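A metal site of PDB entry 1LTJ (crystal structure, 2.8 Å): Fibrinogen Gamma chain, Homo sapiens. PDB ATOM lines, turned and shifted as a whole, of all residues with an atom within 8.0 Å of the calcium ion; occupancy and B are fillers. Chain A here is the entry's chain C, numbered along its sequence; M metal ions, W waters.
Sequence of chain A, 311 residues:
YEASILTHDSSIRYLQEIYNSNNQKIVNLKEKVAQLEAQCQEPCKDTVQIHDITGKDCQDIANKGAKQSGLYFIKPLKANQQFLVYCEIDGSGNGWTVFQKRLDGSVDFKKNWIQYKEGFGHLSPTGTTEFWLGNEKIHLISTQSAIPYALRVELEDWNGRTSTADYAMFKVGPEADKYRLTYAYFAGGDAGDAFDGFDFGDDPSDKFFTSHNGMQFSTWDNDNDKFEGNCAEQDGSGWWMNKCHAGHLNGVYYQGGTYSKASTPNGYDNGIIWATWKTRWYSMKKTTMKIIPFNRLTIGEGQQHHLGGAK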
ATOM      1  N   SER A 218       8.526   5.412   3.668  1.00  0.00           N
ATOM      2  CA  SER A 218       7.996   5.338   2.310  1.00  0.00           C
ATOM      3  C   SER A 218       7.496   6.689   1.824  1.00  0.00           C
ATOM      4  O   SER A 218       7.083   7.533   2.621  1.00  0.00           O
ATOM      5  CB  SER A 218       6.855   4.317   2.265  1.00  0.00           C
ATOM      6  OG  SER A 218       7.115   3.168   3.070  1.00  0.00           O
ATOM      7  N   ASN A 222       8.807   6.415  -3.891  1.00  0.00           N
ATOM      8  CA  ASN A 222       9.655   5.360  -3.340  1.00  0.00           C
ATOM      9  C   ASN A 222       8.843   4.531  -2.351  1.00  0.00           C
ATOM     10  O   ASN A 222       8.909   4.754  -1.143  1.00  0.00           O
ATOM     11  CB  ASN A 222      10.883   5.968  -2.663  1.00  0.00           C
ATOM     12  CG  ASN A 222      11.974   4.935  -2.386  1.00  0.00           C
ATOM     13  OD1 ASN A 222      13.155   5.190  -2.616  1.00  0.00           O
ATOM     14  ND2 ASN A 222      11.576   3.767  -1.887  1.00  0.00           N
ATOM     15  N   ASP A 223       8.081   3.582  -2.892  1.00  0.00           N
ATOM     16  CA  ASP A 223       7.212   2.699  -2.108  1.00  0.00           C
ATOM     17  C   ASP A 223       7.974   1.564  -1.416  1.00  0.00           C
ATOM     18  O   ASP A 223       8.623   0.743  -2.092  1.00  0.00           O
ATOM     19  CB  ASP A 223       6.139   2.100  -3.024  1.00  0.00           C
ATOM     20  CG  ASP A 223       5.077   1.342  -2.267  1.00  0.00           C
ATOM     21  OD1 ASP A 223       5.439   0.494  -1.425  1.00  0.00           O
ATOM     22  OD2 ASP A 223       3.878   1.591  -2.516  1.00  0.00           O
ATOM     23  N   ASN A 224       7.902   1.518  -0.098  1.00  0.00           N
ATOM     24  CA  ASN A 224       8.568   0.468   0.663  1.00  0.00           C
ATOM     25  C   ASN A 224       7.625  -0.078   1.728  1.00  0.00           C
ATOM     26  O   ASN A 224       8.069  -0.586   2.753  1.00  0.00           O
ATOM     27  CB  ASN A 224       9.841   0.996   1.351  1.00  0.00           C
ATOM     28  CG  ASN A 224      10.807   1.645   0.362  1.00  0.00           C
ATOM     29  OD1 ASN A 224      10.988   2.858   0.368  1.00  0.00           O
ATOM     30  ND2 ASN A 224      11.439   0.836  -0.472  1.00  0.00           N
ATOM     31  N   ASP A 225       6.328   0.029   1.480  1.00  0.00           N
ATOM     32  CA  ASP A 225       5.344  -0.451   2.438  1.00  0.00           C
ATOM     33  C   ASP A 225       4.882  -1.857   2.140  1.00  0.00           C
ATOM     34  O   ASP A 225       5.163  -2.411   1.087  1.00  0.00           O
ATOM     35  CB  ASP A 225       4.146   0.495   2.509  1.00  0.00           C
ATOM     36  CG  ASP A 225       3.327   0.496   1.231  1.00  0.00           C
ATOM     37  OD1 ASP A 225       3.224  -0.570   0.578  1.00  0.00           O
ATOM     38  OD2 ASP A 225       2.778   1.568   0.880  1.00  0.00           O
ATOM     39  N   LYS A 226       4.143  -2.435   3.094  1.00  0.00           N
ATOM     40  CA  LYS A 226       3.613  -3.783   2.950  1.00  0.00           C
ATOM     41  C   LYS A 226       2.183  -3.726   2.415  1.00  0.00           C
ATOM     42  O   LYS A 226       1.238  -4.072   3.123  1.00  0.00           O
ATOM     43  CB  LYS A 226       3.615  -4.484   4.313  1.00  0.00           C
ATOM     44  CG  LYS A 226       4.909  -4.373   5.106  1.00  0.00           C
ATOM     45  CD  LYS A 226       6.100  -4.966   4.382  1.00  0.00           C
ATOM     46  CE  LYS A 226       7.318  -4.996   5.300  1.00  0.00           C
ATOM     47  NZ  LYS A 226       8.566  -5.372   4.578  1.00  0.00           N
ATOM     48  N   PHE A 227       2.028  -3.301   1.162  1.00  0.00           N
ATOM     49  CA  PHE A 227       0.707  -3.182   0.544  1.00  0.00           C
ATOM     50  C   PHE A 227       0.888  -2.970  -0.944  1.00  0.00           C
ATOM     51  O   PHE A 227       1.605  -2.082  -1.371  1.00  0.00           O
ATOM     52  CB  PHE A 227      -0.039  -1.996   1.172  1.00  0.00           C
ATOM     53  CG  PHE A 227      -1.238  -1.536   0.396  1.00  0.00           C
ATOM     54  CD1 PHE A 227      -2.241  -2.423   0.051  1.00  0.00           C
ATOM     55  CD2 PHE A 227      -1.378  -0.194   0.058  1.00  0.00           C
ATOM     56  CE1 PHE A 227      -3.378  -1.981  -0.630  1.00  0.00           C
ATOM     57  CE2 PHE A 227      -2.516   0.265  -0.617  1.00  0.00           C
ATOM     58  CZ  PHE A 227      -3.510  -0.627  -0.965  1.00  0.00           C
ATOM     59  N   GLU A 228       0.238  -3.822  -1.738  1.00  0.00           N
ATOM     60  CA  GLU A 228       0.337  -3.745  -3.188  1.00  0.00           C
ATOM     61  C   GLU A 228       0.151  -2.316  -3.677  1.00  0.00           C
ATOM     62  O   GLU A 228       0.717  -1.916  -4.681  1.00  0.00           O
ATOM     63  CB  GLU A 228      -0.723  -4.640  -3.836  1.00  0.00           C
ATOM     64  CG  GLU A 228      -2.136  -4.136  -3.615  1.00  0.00           C
ATOM     65  CD  GLU A 228      -3.153  -4.891  -4.444  1.00  0.00           C
ATOM     66  OE1 GLU A 228      -4.290  -4.386  -4.572  1.00  0.00           O
ATOM     67  OE2 GLU A 228      -2.826  -5.981  -4.959  1.00  0.00           O
ATOM     68  N   GLY A 229      -0.674  -1.565  -2.961  1.00  0.00           N
ATOM     69  CA  GLY A 229      -0.909  -0.188  -3.345  1.00  0.00           C
ATOM     70  C   GLY A 229       0.176   0.712  -2.829  1.00  0.00           C
ATOM     71  O   GLY A 229       1.200   0.242  -2.319  1.00  0.00           O
ATOM     72  N   ASN A 230      -0.020   2.012  -2.936  1.00  0.00           N
ATOM     73  CA  ASN A 230       0.976   2.963  -2.477  1.00  0.00           C
ATOM     74  C   ASN A 230       0.436   3.827  -1.345  1.00  0.00           C
ATOM     75  O   ASN A 230      -0.143   4.887  -1.596  1.00  0.00           O
ATOM     76  CB  ASN A 230       1.429   3.833  -3.656  1.00  0.00           C
ATOM     77  CG  ASN A 230       2.653   4.657  -3.329  1.00  0.00           C
ATOM     78  OD1 ASN A 230       3.295   5.214  -4.226  1.00  0.00           O
ATOM     79  ND2 ASN A 230       2.981   4.763  -2.051  1.00  0.00           N
ATOM     80  N   CYS A 231       0.634   3.363  -0.113  1.00  0.00           N
ATOM     81  CA  CYS A 231       0.168   4.088   1.063  1.00  0.00           C
ATOM     82  C   CYS A 231       0.551   5.555   0.964  1.00  0.00           C
ATOM     83  O   CYS A 231      -0.313   6.418   0.868  1.00  0.00           O
ATOM     84  CB  CYS A 231       0.779   3.513   2.345  1.00  0.00           C
ATOM     85  SG  CYS A 231       0.249   1.841   2.858  1.00  0.00           S
ATOM     86  N   ALA A 232       1.860   5.799   0.965  1.00  0.00           N
ATOM     87  CA  ALA A 232       2.396   7.160   0.884  1.00  0.00           C
ATOM     88  C   ALA A 232       1.718   8.000  -0.189  1.00  0.00           C
ATOM     89  O   ALA A 232       1.468   9.190   0.004  1.00  0.00           O
ATOM     90  CB  ALA A 232       3.892   7.102   0.632  1.00  0.00           C
ATOM     91  N   MET A 241       5.201   3.621   6.418  1.00  0.00           N
ATOM     92  CA  MET A 241       3.977   2.904   6.067  1.00  0.00           C
ATOM     93  C   MET A 241       4.058   1.386   6.143  1.00  0.00           C
ATOM     94  O   MET A 241       5.110   0.781   5.927  1.00  0.00           O
ATOM     95  CB  MET A 241       3.528   3.306   4.665  1.00  0.00           C
ATOM     96  CG  MET A 241       3.185   4.765   4.512  1.00  0.00           C
ATOM     97  SD  MET A 241       1.716   5.176   5.455  1.00  0.00           S
ATOM     98  CE  MET A 241       0.854   6.223   4.297  1.00  0.00           C
ATOM     99  N   ASN A 242       2.902   0.797   6.437  1.00  0.00           N
ATOM    100  CA  ASN A 242       2.710  -0.655   6.550  1.00  0.00           C
ATOM    101  C   ASN A 242       1.586  -0.989   5.566  1.00  0.00           C
ATOM    102  O   ASN A 242       1.832  -1.248   4.384  1.00  0.00           O
ATOM    103  CB  ASN A 242       2.313  -0.994   7.990  1.00  0.00           C
ATOM    104  CG  ASN A 242       2.157  -2.487   8.227  1.00  0.00           C
ATOM    105  OD1 ASN A 242       1.459  -3.178   7.489  1.00  0.00           O
ATOM    106  ND2 ASN A 242       2.798  -2.977   9.274  1.00  0.00           N
ATOM    107  N   LYS A 243       0.338  -0.980   6.042  1.00  0.00           N
ATOM    108  CA  LYS A 243      -0.825  -1.236   5.198  1.00  0.00           C
ATOM    109  C   LYS A 243      -2.133  -0.832   5.880  1.00  0.00           C
ATOM    110  O   LYS A 243      -3.035  -1.657   6.038  1.00  0.00           O
ATOM    111  CB  LYS A 243      -0.918  -2.716   4.783  1.00  0.00           C
ATOM    112  CG  LYS A 243      -1.949  -2.957   3.661  1.00  0.00           C
ATOM    113  CD  LYS A 243      -1.882  -4.355   3.045  1.00  0.00           C
ATOM    114  CE  LYS A 243      -2.714  -5.359   3.811  1.00  0.00           C
ATOM    115  NZ  LYS A 243      -4.142  -4.928   3.873  1.00  0.00           N
ATOM    116  N   CYS A 244      -2.231   0.428   6.288  1.00  0.00           N
ATOM    117  CA  CYS A 244      -1.161   1.396   6.087  1.00  0.00           C
ATOM    118  C   CYS A 244      -0.650   2.020   7.377  1.00  0.00           C
ATOM    119  O   CYS A 244       0.554   1.975   7.640  1.00  0.00           O
ATOM    120  CB  CYS A 244      -1.604   2.516   5.155  1.00  0.00           C
ATOM    121  SG  CYS A 244      -1.698   2.089   3.389  1.00  0.00           S
HETATM  122 CA    CA M   1       3.261  -0.913  -1.852  1.00  0.00          CA
HETATM  123  O   HOH W   1       5.082  -2.230  -1.287  1.00  0.00           O
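C of Glu 228 touches the calcium ion, at 3.9 Å.
OD2 of Asp 223 sits close to ND2 of Asn 230. The side-chain sulfur of Cys 231 forms a disulfide with the side-chain sulfur of Cys 244, at 2.0 Å. N of Cys 231 is in hydrogen-bond range of OD2 of Asp 225 (3.0 Å).
The calcium ion is bound by the backbone carbonyl oxygen (O) of Phe 227 (2.1 Å), water W1 (2.3 Å), the backbone carbonyl oxygen (O) of Gly 229 (2.4 Å), the side-chain carboxylate (OD1) of Asp 225 (2.5 Å), the side-chain carboxylate (OD1) of Asp 223 (2.6 Å) and the side-chain carboxylate (OD2) of Asp 223 (2.7 Å). The calcium ion has six donor atoms within binding distance.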
